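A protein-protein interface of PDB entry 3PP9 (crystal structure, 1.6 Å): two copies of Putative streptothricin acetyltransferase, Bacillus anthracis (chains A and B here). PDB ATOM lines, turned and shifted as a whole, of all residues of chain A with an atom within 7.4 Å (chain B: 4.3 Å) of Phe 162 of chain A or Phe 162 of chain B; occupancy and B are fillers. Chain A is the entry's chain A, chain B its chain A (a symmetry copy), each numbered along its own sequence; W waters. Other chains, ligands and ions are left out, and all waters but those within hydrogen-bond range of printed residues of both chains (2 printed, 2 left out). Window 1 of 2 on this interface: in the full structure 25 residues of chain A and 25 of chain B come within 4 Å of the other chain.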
ATOM      1  N   LEU A  34      11.432  29.948 -24.120  1.00  0.00           N
ATOM      2  CA  LEU A  34      10.179  29.210 -24.248  1.00  0.00           C
ATOM      3  C   LEU A  34       9.226  29.200 -23.072  1.00  0.00           C
ATOM      4  O   LEU A  34       9.627  29.318 -21.908  1.00  0.00           O
ATOM      5  CB  LEU A  34      10.542  27.755 -24.588  1.00  0.00           C
ATOM      6  CG  LEU A  34      11.398  27.563 -25.839  1.00  0.00           C
ATOM      7  CD1 LEU A  34      11.838  26.130 -25.945  1.00  0.00           C
ATOM      8  CD2 LEU A  34      10.671  27.991 -27.089  1.00  0.00           C
ATOM      9  N   SER A  35       7.939  29.101 -23.400  1.00  0.00           N
ATOM     10  CA  SER A  35       6.890  29.009 -22.397  1.00  0.00           C
ATOM     11  C   SER A  35       5.822  28.059 -22.931  1.00  0.00           C
ATOM     12  O   SER A  35       5.742  27.803 -24.142  1.00  0.00           O
ATOM     13  CB  SER A  35       6.282  30.369 -22.056  1.00  0.00           C
ATOM     14  OG  SER A  35       5.691  30.964 -23.195  1.00  0.00           O
ATOM     15  N   LEU A  36       5.024  27.511 -22.019  1.00  0.00           N
ATOM     16  CA  LEU A  36       3.973  26.558 -22.368  1.00  0.00           C
ATOM     17  C   LEU A  36       2.632  27.047 -21.846  1.00  0.00           C
ATOM     18  O   LEU A  36       2.419  27.124 -20.631  1.00  0.00           O
ATOM     19  CB  LEU A  36       4.286  25.187 -21.757  1.00  0.00           C
ATOM     20  CG  LEU A  36       3.285  24.064 -22.030  1.00  0.00           C
ATOM     21  CD1 LEU A  36       3.151  23.856 -23.521  1.00  0.00           C
ATOM     22  CD2 LEU A  36       3.693  22.756 -21.353  1.00  0.00           C
ATOM     23  N   ARG A  41      -1.914  23.299 -25.496  1.00  0.00           N
ATOM     24  CA  ARG A  41      -0.499  22.935 -25.324  1.00  0.00           C
ATOM     25  C   ARG A  41       0.412  23.744 -26.255  1.00  0.00           C
ATOM     26  O   ARG A  41       1.423  23.243 -26.761  1.00  0.00           O
ATOM     27  CB  ARG A  41      -0.334  21.432 -25.587  1.00  0.00           C
ATOM     28  CG  ARG A  41      -1.327  20.579 -24.783  1.00  0.00           C
ATOM     29  CD  ARG A  41      -1.182  19.069 -24.988  1.00  0.00           C
ATOM     30  NE  ARG A  41      -1.226  18.667 -26.391  1.00  0.00           N
ATOM     31  CZ  ARG A  41      -1.239  17.401 -26.801  1.00  0.00           C
ATOM     32  NH1 ARG A  41      -1.271  17.120 -28.096  1.00  0.00           N
ATOM     33  NH2 ARG A  41      -1.228  16.413 -25.918  1.00  0.00           N
ATOM     34  N   ARG A  42       0.061  25.010 -26.453  1.00  0.00           N
ATOM     35  CA  ARG A  42       0.800  25.875 -27.339  1.00  0.00           C
ATOM     36  C   ARG A  42       2.100  26.322 -26.694  1.00  0.00           C
ATOM     37  O   ARG A  42       2.110  26.865 -25.585  1.00  0.00           O
ATOM     38  CB  ARG A  42      -0.050  27.101 -27.672  1.00  0.00           C
ATOM     39  CG  ARG A  42       0.503  28.019 -28.744  1.00  0.00           C
ATOM     40  CD  ARG A  42      -0.347  29.283 -28.841  1.00  0.00           C
ATOM     41  NE  ARG A  42       0.031  30.090 -29.999  1.00  0.00           N
ATOM     42  CZ  ARG A  42      -0.500  29.952 -31.215  1.00  0.00           C
ATOM     43  NH1 ARG A  42      -1.427  29.028 -31.452  1.00  0.00           N
ATOM     44  NH2 ARG A  42      -0.092  30.735 -32.211  1.00  0.00           N
ATOM     45  N   ILE A  43       3.188  26.068 -27.399  1.00  0.00           N
ATOM     46  CA  ILE A  43       4.502  26.469 -26.952  1.00  0.00           C
ATOM     47  C   ILE A  43       4.724  27.840 -27.549  1.00  0.00           C
ATOM     48  O   ILE A  43       4.619  28.029 -28.767  1.00  0.00           O
ATOM     49  CB  ILE A  43       5.591  25.508 -27.426  1.00  0.00           C
ATOM     50  CG1 ILE A  43       5.401  24.146 -26.754  1.00  0.00           C
ATOM     51  CG2 ILE A  43       6.972  26.079 -27.093  1.00  0.00           C
ATOM     52  CD1 ILE A  43       6.327  23.060 -27.280  1.00  0.00           C
ATOM     53  N   GLU A  44       5.026  28.800 -26.691  1.00  0.00           N
ATOM     54  CA  GLU A  44       5.238  30.155 -27.133  1.00  0.00           C
ATOM     55  C   GLU A  44       6.653  30.565 -26.816  1.00  0.00           C
ATOM     56  O   GLU A  44       7.396  29.860 -26.139  1.00  0.00           O
ATOM     57  CB  GLU A  44       4.264  31.090 -26.421  1.00  0.00           C
ATOM     58  CG  GLU A  44       2.809  30.776 -26.706  1.00  0.00           C
ATOM     59  CD  GLU A  44       1.852  31.671 -25.950  1.00  0.00           C
ATOM     60  OE1 GLU A  44       2.248  32.252 -24.916  1.00  0.00           O
ATOM     61  OE2 GLU A  44       0.686  31.768 -26.381  1.00  0.00           O
ATOM     62  N   ILE A 159       6.171  25.146 -33.396  1.00  0.00           N
ATOM     63  CA  ILE A 159       6.964  24.436 -32.397  1.00  0.00           C
ATOM     64  C   ILE A 159       6.113  23.343 -31.748  1.00  0.00           C
ATOM     65  O   ILE A 159       5.025  23.610 -31.227  1.00  0.00           O
ATOM     66  CB  ILE A 159       7.453  25.367 -31.302  1.00  0.00           C
ATOM     67  CG1 ILE A 159       8.364  26.439 -31.902  1.00  0.00           C
ATOM     68  CG2 ILE A 159       8.220  24.560 -30.264  1.00  0.00           C
ATOM     69  CD1 ILE A 159       8.842  27.461 -30.894  1.00  0.00           C
ATOM     70  N   GLY A 160       6.630  22.112 -31.793  1.00  0.00           N
ATOM     71  CA  GLY A 160       5.949  20.975 -31.200  1.00  0.00           C
ATOM     72  C   GLY A 160       6.597  20.456 -29.930  1.00  0.00           C
ATOM     73  O   GLY A 160       5.977  19.725 -29.181  1.00  0.00           O
ATOM     74  N   GLY A 161       7.846  20.833 -29.689  1.00  0.00           N
ATOM     75  CA  GLY A 161       8.529  20.367 -28.499  1.00  0.00           C
ATOM     76  C   GLY A 161       9.862  21.045 -28.299  1.00  0.00           C
ATOM     77  O   GLY A 161      10.299  21.819 -29.137  1.00  0.00           O
ATOM     78  N   PHE A 162      10.489  20.759 -27.166  1.00  0.00           N
ATOM     79  CA  PHE A 162      11.786  21.347 -26.846  1.00  0.00           C
ATOM     80  C   PHE A 162      12.478  20.470 -25.821  1.00  0.00           C
ATOM     81  O   PHE A 162      11.846  19.610 -25.193  1.00  0.00           O
ATOM     82  CB  PHE A 162      11.693  22.835 -26.439  1.00  0.00           C
ATOM     83  CG  PHE A 162      10.715  23.156 -25.349  1.00  0.00           C
ATOM     84  CD1 PHE A 162      11.033  22.947 -24.020  1.00  0.00           C
ATOM     85  CD2 PHE A 162       9.525  23.808 -25.657  1.00  0.00           C
ATOM     86  CE1 PHE A 162      10.129  23.310 -23.015  1.00  0.00           C
ATOM     87  CE2 PHE A 162       8.622  24.173 -24.666  1.00  0.00           C
ATOM     88  CZ  PHE A 162       8.924  23.920 -23.351  1.00  0.00           C
ATOM     89  N   ASP A 163      13.772  20.677 -25.651  1.00  0.00           N
ATOM     90  CA  ASP A 163      14.528  19.870 -24.711  1.00  0.00           C
ATOM     91  C   ASP A 163      15.676  20.701 -24.130  1.00  0.00           C
ATOM     92  O   ASP A 163      16.558  21.168 -24.857  1.00  0.00           O
ATOM     93  CB  ASP A 163      15.025  18.607 -25.405  1.00  0.00           C
ATOM     94  CG  ASP A 163      15.566  17.594 -24.449  1.00  0.00           C
ATOM     95  OD1 ASP A 163      16.407  17.973 -23.611  1.00  0.00           O
ATOM     96  OD2 ASP A 163      15.165  16.404 -24.579  1.00  0.00           O
ATOM     97  N   PHE A 164      15.648  20.836 -22.814  1.00  0.00           N
ATOM     98  CA  PHE A 164      16.632  21.611 -22.057  1.00  0.00           C
ATOM     99  C   PHE A 164      17.889  20.868 -21.642  1.00  0.00           C
ATOM    100  O   PHE A 164      18.853  21.519 -21.204  1.00  0.00           O
ATOM    101  CB  PHE A 164      16.039  22.107 -20.722  1.00  0.00           C
ATOM    102  CG  PHE A 164      14.829  22.976 -20.859  1.00  0.00           C
ATOM    103  CD1 PHE A 164      14.910  24.199 -21.496  1.00  0.00           C
ATOM    104  CD2 PHE A 164      13.641  22.625 -20.242  1.00  0.00           C
ATOM    105  CE1 PHE A 164      13.791  25.033 -21.600  1.00  0.00           C
ATOM    106  CE2 PHE A 164      12.520  23.457 -20.328  1.00  0.00           C
ATOM    107  CZ  PHE A 164      12.610  24.669 -21.016  1.00  0.00           C
ATOM    108  N   LEU A 165      17.913  19.545 -21.760  1.00  0.00           N
ATOM    109  CA  LEU A 165      19.062  18.792 -21.299  1.00  0.00           C
ATOM    110  C   LEU A 165      19.842  18.033 -22.350  1.00  0.00           C
ATOM    111  O   LEU A 165      20.990  17.662 -22.091  1.00  0.00           O
ATOM    112  CB  LEU A 165      18.614  17.803 -20.212  1.00  0.00           C
ATOM    113  CG  LEU A 165      18.012  18.422 -18.939  1.00  0.00           C
ATOM    114  CD1 LEU A 165      17.603  17.350 -17.927  1.00  0.00           C
ATOM    115  CD2 LEU A 165      18.980  19.380 -18.278  1.00  0.00           C
ATOM    116  N   VAL A 166      19.270  17.826 -23.525  1.00  0.00           N
ATOM    117  CA  VAL A 166      19.975  17.006 -24.526  1.00  0.00           C
ATOM    118  C   VAL A 166      21.384  17.564 -24.841  1.00  0.00           C
ATOM    119  O   VAL A 166      22.377  16.816 -24.906  1.00  0.00           O
ATOM    120  CB  VAL A 166      19.125  16.731 -25.754  1.00  0.00           C
ATOM    121  CG1 VAL A 166      18.876  17.997 -26.588  1.00  0.00           C
ATOM    122  CG2 VAL A 166      19.771  15.594 -26.596  1.00  0.00           C
ATOM    123  N   VAL A 177      19.092  25.068 -25.889  1.00  0.00           N
ATOM    124  CA  VAL A 177      17.822  24.335 -25.866  1.00  0.00           C
ATOM    125  C   VAL A 177      17.473  23.881 -27.274  1.00  0.00           C
ATOM    126  O   VAL A 177      17.566  24.659 -28.225  1.00  0.00           O
ATOM    127  CB  VAL A 177      16.668  25.235 -25.351  1.00  0.00           C
ATOM    128  CG1 VAL A 177      15.343  24.475 -25.262  1.00  0.00           C
ATOM    129  CG2 VAL A 177      17.016  25.861 -23.969  1.00  0.00           C
ATOM    130  N   ALA A 178      17.105  22.611 -27.419  1.00  0.00           N
ATOM    131  CA  ALA A 178      16.681  22.074 -28.710  1.00  0.00           C
ATOM    132  C   ALA A 178      15.215  22.420 -28.902  1.00  0.00           C
ATOM    133  O   ALA A 178      14.414  22.293 -27.965  1.00  0.00           O
ATOM    134  CB  ALA A 178      16.831  20.541 -28.724  1.00  0.00           C
ATOM    135  N   ILE A 179      14.862  22.868 -30.105  1.00  0.00           N
ATOM    136  CA  ILE A 179      13.495  23.215 -30.452  1.00  0.00           C
ATOM    137  C   ILE A 179      13.098  22.362 -31.656  1.00  0.00           C
ATOM    138  O   ILE A 179      13.819  22.308 -32.654  1.00  0.00           O
ATOM    139  CB  ILE A 179      13.311  24.705 -30.781  1.00  0.00           C
ATOM    140  CG1 ILE A 179      13.792  25.571 -29.613  1.00  0.00           C
ATOM    141  CG2 ILE A 179      11.846  24.993 -31.094  1.00  0.00           C
ATOM    142  CD1 ILE A 179      13.643  27.076 -29.851  1.00  0.00           C
ATOM    143  N   TYR A 180      11.959  21.698 -31.548  1.00  0.00           N
ATOM    144  CA  TYR A 180      11.460  20.819 -32.629  1.00  0.00           C
ATOM    145  C   TYR A 180      10.286  21.489 -33.366  1.00  0.00           C
ATOM    146  O   TYR A 180       9.281  21.844 -32.751  1.00  0.00           O
ATOM    147  CB  TYR A 180      11.124  19.455 -32.038  1.00  0.00           C
ATOM    148  CG  TYR A 180      12.340  18.905 -31.329  1.00  0.00           C
ATOM    149  CD1 TYR A 180      13.314  18.211 -32.013  1.00  0.00           C
ATOM    150  CD2 TYR A 180      12.524  19.133 -29.976  1.00  0.00           C
ATOM    151  CE1 TYR A 180      14.450  17.729 -31.343  1.00  0.00           C
ATOM    152  CE2 TYR A 180      13.639  18.655 -29.312  1.00  0.00           C
ATOM    153  CZ  TYR A 180      14.591  17.973 -29.996  1.00  0.00           C
ATOM    154  OH  TYR A 180      15.686  17.517 -29.291  1.00  0.00           O
ATOM    155  N   TYR A 182       7.547  21.621 -36.716  1.00  0.00           N
ATOM    156  CA  TYR A 182       6.713  20.760 -37.532  1.00  0.00           C
ATOM    157  C   TYR A 182       5.827  21.491 -38.513  1.00  0.00           C
ATOM    158  O   TYR A 182       5.250  22.511 -38.180  1.00  0.00           O
ATOM    159  CB  TYR A 182       5.760  19.983 -36.591  1.00  0.00           C
ATOM    160  CG  TYR A 182       6.508  19.066 -35.651  1.00  0.00           C
ATOM    161  CD1 TYR A 182       6.732  17.738 -35.971  1.00  0.00           C
ATOM    162  CD2 TYR A 182       7.049  19.547 -34.467  1.00  0.00           C
ATOM    163  CE1 TYR A 182       7.478  16.910 -35.128  1.00  0.00           C
ATOM    164  CE2 TYR A 182       7.794  18.719 -33.628  1.00  0.00           C
ATOM    165  CZ  TYR A 182       7.968  17.400 -33.948  1.00  0.00           C
ATOM    166  OH  TYR A 182       8.745  16.613 -33.116  1.00  0.00           O
ATOM    167  N   LEU B  34       1.862  17.625 -18.564  1.00  0.00           N
ATOM    168  CA  LEU B  34       3.042  18.458 -18.352  1.00  0.00           C
ATOM    169  C   LEU B  34       2.852  19.952 -18.205  1.00  0.00           C
ATOM    170  O   LEU B  34       1.904  20.543 -18.736  1.00  0.00           O
ATOM    171  CB  LEU B  34       3.994  18.206 -19.533  1.00  0.00           C
ATOM    172  CG  LEU B  34       4.406  16.751 -19.750  1.00  0.00           C
ATOM    173  CD1 LEU B  34       5.170  16.621 -21.038  1.00  0.00           C
ATOM    174  CD2 LEU B  34       5.215  16.217 -18.595  1.00  0.00           C
ATOM    175  N   LEU B  36       5.451  23.724 -17.401  1.00  0.00           N
ATOM    176  CA  LEU B  36       6.795  24.296 -17.392  1.00  0.00           C
ATOM    177  C   LEU B  36       6.854  25.471 -16.430  1.00  0.00           C
ATOM    178  O   LEU B  36       6.213  26.503 -16.657  1.00  0.00           O
ATOM    179  CB  LEU B  36       7.170  24.773 -18.800  1.00  0.00           C
ATOM    180  CG  LEU B  36       8.556  25.397 -18.972  1.00  0.00           C
ATOM    181  CD1 LEU B  36       9.615  24.404 -18.551  1.00  0.00           C
ATOM    182  CD2 LEU B  36       8.805  25.852 -20.409  1.00  0.00           C
ATOM    183  N   ILE B  43      10.399  21.125 -15.624  1.00  0.00           N
ATOM    184  CA  ILE B  43       9.222  20.546 -16.230  1.00  0.00           C
ATOM    185  C   ILE B  43       8.570  19.735 -15.134  1.00  0.00           C
ATOM    186  O   ILE B  43       9.200  18.862 -14.525  1.00  0.00           O
ATOM    187  CB  ILE B  43       9.567  19.645 -17.415  1.00  0.00           C
ATOM    188  CG1 ILE B  43      10.155  20.491 -18.547  1.00  0.00           C
ATOM    189  CG2 ILE B  43       8.312  18.911 -17.894  1.00  0.00           C
ATOM    190  CD1 ILE B  43      10.692  19.678 -19.715  1.00  0.00           C
ATOM    191  N   GLY B 161      12.748  17.260 -21.445  1.00  0.00           N
ATOM    192  CA  GLY B 161      12.022  17.784 -22.584  1.00  0.00           C
ATOM    193  C   GLY B 161      10.799  16.964 -22.911  1.00  0.00           C
ATOM    194  O   GLY B 161      10.561  15.931 -22.304  1.00  0.00           O
ATOM    195  N   PHE B 162      10.016  17.451 -23.864  1.00  0.00           N
ATOM    196  CA  PHE B 162       8.800  16.758 -24.278  1.00  0.00           C
ATOM    197  C   PHE B 162       8.428  17.220 -25.673  1.00  0.00           C
ATOM    198  O   PHE B 162       8.940  18.235 -26.162  1.00  0.00           O
ATOM    199  CB  PHE B 162       7.653  16.881 -23.250  1.00  0.00           C
ATOM    200  CG  PHE B 162       7.312  18.273 -22.812  1.00  0.00           C
ATOM    201  CD1 PHE B 162       6.522  19.094 -23.595  1.00  0.00           C
ATOM    202  CD2 PHE B 162       7.667  18.705 -21.538  1.00  0.00           C
ATOM    203  CE1 PHE B 162       6.165  20.369 -23.141  1.00  0.00           C
ATOM    204  CE2 PHE B 162       7.316  19.968 -21.078  1.00  0.00           C
ATOM    205  CZ  PHE B 162       6.571  20.796 -21.880  1.00  0.00           C
ATOM    206  N   ASP B 163       7.545  16.478 -26.320  1.00  0.00           N
ATOM    207  CA  ASP B 163       7.145  16.823 -27.671  1.00  0.00           C
ATOM    208  C   ASP B 163       5.698  16.382 -27.905  1.00  0.00           C
ATOM    209  O   ASP B 163       5.370  15.194 -27.820  1.00  0.00           O
ATOM    210  CB  ASP B 163       8.109  16.190 -28.668  1.00  0.00           C
ATOM    211  CG  ASP B 163       7.940  16.719 -30.055  1.00  0.00           C
ATOM    212  OD1 ASP B 163       6.791  16.740 -30.536  1.00  0.00           O
ATOM    213  OD2 ASP B 163       8.985  17.074 -30.669  1.00  0.00           O
ATOM    214  N   PHE B 164       4.868  17.360 -28.229  1.00  0.00           N
ATOM    215  CA  PHE B 164       3.438  17.164 -28.468  1.00  0.00           C
ATOM    216  C   PHE B 164       3.045  16.784 -29.886  1.00  0.00           C
ATOM    217  O   PHE B 164       1.889  16.384 -30.101  1.00  0.00           O
ATOM    218  CB  PHE B 164       2.648  18.464 -28.204  1.00  0.00           C
ATOM    219  CG  PHE B 164       2.775  19.000 -26.813  1.00  0.00           C
ATOM    220  CD1 PHE B 164       2.311  18.275 -25.734  1.00  0.00           C
ATOM    221  CD2 PHE B 164       3.245  20.285 -26.599  1.00  0.00           C
ATOM    222  CE1 PHE B 164       2.397  18.783 -24.433  1.00  0.00           C
ATOM    223  CE2 PHE B 164       3.322  20.808 -25.304  1.00  0.00           C
ATOM    224  CZ  PHE B 164       2.890  20.040 -24.221  1.00  0.00           C
ATOM    225  N   VAL B 177       2.173  12.155 -26.020  1.00  0.00           N
ATOM    226  CA  VAL B 177       3.272  13.111 -25.845  1.00  0.00           C
ATOM    227  C   VAL B 177       4.550  12.358 -25.513  1.00  0.00           C
ATOM    228  O   VAL B 177       4.548  11.462 -24.667  1.00  0.00           O
ATOM    229  CB  VAL B 177       2.976  14.094 -24.683  1.00  0.00           C
ATOM    230  CG1 VAL B 177       4.082  15.138 -24.517  1.00  0.00           C
ATOM    231  CG2 VAL B 177       1.602  14.800 -24.877  1.00  0.00           C
ATOM    232  N   ALA B 178       5.638  12.694 -26.201  1.00  0.00           N
ATOM    233  CA  ALA B 178       6.940  12.090 -25.926  1.00  0.00           C
ATOM    234  C   ALA B 178       7.565  12.837 -24.761  1.00  0.00           C
ATOM    235  O   ALA B 178       7.510  14.074 -24.708  1.00  0.00           O
ATOM    236  CB  ALA B 178       7.861  12.232 -27.152  1.00  0.00           C
ATOM    237  N   TYR B 180      11.191  13.079 -22.543  1.00  0.00           N
ATOM    238  CA  TYR B 180      12.630  12.737 -22.550  1.00  0.00           C
ATOM    239  C   TYR B 180      13.213  12.834 -21.128  1.00  0.00           C
ATOM    240  O   TYR B 180      13.135  13.885 -20.491  1.00  0.00           O
ATOM    241  CB  TYR B 180      13.339  13.616 -23.574  1.00  0.00           C
ATOM    242  CG  TYR B 180      12.674  13.450 -24.920  1.00  0.00           C
ATOM    243  CD1 TYR B 180      13.025  12.423 -25.769  1.00  0.00           C
ATOM    244  CD2 TYR B 180      11.657  14.305 -25.308  1.00  0.00           C
ATOM    245  CE1 TYR B 180      12.379  12.270 -27.007  1.00  0.00           C
ATOM    246  CE2 TYR B 180      11.022  14.159 -26.528  1.00  0.00           C
ATOM    247  CZ  TYR B 180      11.376  13.145 -27.357  1.00  0.00           C
ATOM    248  OH  TYR B 180      10.714  13.039 -28.563  1.00  0.00           O
HETATM  249  O   HOH W   1       5.439  28.182 -19.207  1.00  0.00           O
HETATM  250  O   HOH W   2       3.192  25.446 -18.079  1.00  0.00           O
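The backbone carbonyl oxygen of Gly 160 of chain A sits at hydrogen-bond distance from the backbone NH of Phe 164 of chain B.
The backbone NH of Phe 162 of chain A sits at hydrogen-bond distance from the backbone carbonyl oxygen of Phe 162 of chain B.
The side-chain hydroxyl (OH) of Tyr 182 of chain A is in hydrogen-bond range of the side-chain carboxylate (OD2) of Asp 163 of chain B (2.5 Å).
The backbone carbonyl oxygen (O) of Gly 160 of chain A sits close to the side-chain carboxylate (OD1) of Asp 163 of chain B, at 3.4 Å.
The backbone carbonyl oxygen (O) of Tyr 180 of chain A lies within hydrogen-bond range of the backbone NH (N) of Gly 160 of chain A (2.8 Å).
The backbone NH (N) of Tyr 180 of chain A sits at hydrogen-bond distance from the backbone carbonyl oxygen (O) of Gly 161 of chain A (2.9 Å).
The side-chain carboxylate (OD1) of Asp 163 of chain A sits at hydrogen-bond distance from the backbone NH (N) of Leu 165 of chain A (2.9 Å).
N of Asp 163 of chain A lies within hydrogen-bond range of O of Ala 178 of chain A (2.9 Å).
The backbone carbonyl oxygen (O) of Gly 161 of chain B lies within hydrogen-bond range of the backbone NH (N) of Tyr 180 of chain B, 2.9 Å away.
The backbone NH (N) of Asp 163 of chain B sits at hydrogen-bond distance from the backbone carbonyl oxygen (O) of Ala 178 of chain B.
Among the printed residues, merely in contact across the chains: Phe 162 of chain A with Gly 161 of chain B (3.2 Å), Gly 161 of chain A with Phe 162 of chain B (3.2 Å), Arg 41 of chain A with Phe 164 of chain B (3.4 Å), Arg 41 of chain A with Val 177 of chain B (3.4 Å), Asp 163 of chain A with Tyr 180 of chain B (3.5 Å), Tyr 180 of chain A with Asp 163 of chain B (3.5 Å), Phe 162 of chain A with Leu 36 of chain B (3.5 Å), Leu 36 of chain A with Phe 162 of chain B (3.5 Å), Phe 164 of chain A with Leu 36 of chain B (3.5 Å), Leu 36 of chain A with Phe 164 of chain B (3.5 Å), Leu 34 of chain A with Leu 36 of chain B (3.9 Å), Leu 36 of chain A with Leu 34 of chain B (3.9 Å), Asp 163 of chain A with Gly 161 of chain B (3.9 Å) and Gly 161 of chain A with Asp 163 of chain B (3.9 Å).
Of the printed residues of chain B, Leu 36 of chain A touches Leu 34, Phe 162 and Phe 164.
Of the printed residues of chain B, Arg 41 of chain A touches Phe 164 (3.4 Å) and Val 177 (3.4 Å).
Printed residues of chain B within 4 Å of Gly 161 of chain A: Phe 162 and Asp 163.
Printed residues of chain B within 4 Å of Phe 162 of chain A: Leu 36 (3.5 Å), Gly 161 (3.2 Å) and Phe 162 (3.1 Å).
Of the printed residues of chain B, Phe 164 of chain A touches Leu 36 (3.5 Å).
Of the printed residues of chain A, Leu 34 of chain B touches Leu 36.
Of the printed residues of chain A, Phe 162 of chain B touches Leu 36, Gly 161 and Phe 162.
The nearest printed residue of chain A that does not touch Phe 162 of chain B is Gly 160 of chain A (4.5 Å).
The nearest printed residue of chain B that does not touch Phe 164 of chain A is Ile 43 of chain B (4.2 Å).
Hydrophobic or aromatic side chains of chain B within 4 Å of the printed part of chain A: Leu 36, Phe 162, Phe 164, Val 177 and Tyr 180.
Of the 20 printed residues of chain A, 10 touch a printed residue of chain B.
Hydrophobic or aromatic side chains of chain A that line the printed part of chain B: Leu 36, Phe 162, Phe 164, Tyr 180 and Tyr 182.
Among the printed residues, 18 pairs touch across the chains.
Among the printed residues, no Asp or Glu carboxylate lies within 4 Å of a Lys or Arg side-chain nitrogen of the other chain.
Leu 34 of chain A touches Leu 36 of chain B, and with the chains exchanged Leu 36 of chain A touches Leu 34 of chain B.
Gly 161 of chain A touches Asp 163 of chain B, and with the chains exchanged Asp 163 of chain A touches Gly 161 of chain B.
Phe 162 of chain A touches its own counterpart, Phe 162 of chain B.
Asp 163 of chain A touches Tyr 180 of chain B, and with the chains exchanged Tyr 180 of chain A touches Asp 163 of chain B.
10 positions are printed for both chains.
Of the 18 pairs that touch across the chains among the printed residues, 13 have their exchanged pair printed and touching as well.
Water W1 lies within hydrogen-bond range of the backbone NH of Leu 36 of chain A (2.9 Å) and the backbone carbonyl oxygen of Leu 36 of chain B (3.1 Å).
Water W2 bridges the backbone NH of Leu 36 of chain B and the backbone carbonyl oxygen of Leu 36 of chain A.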
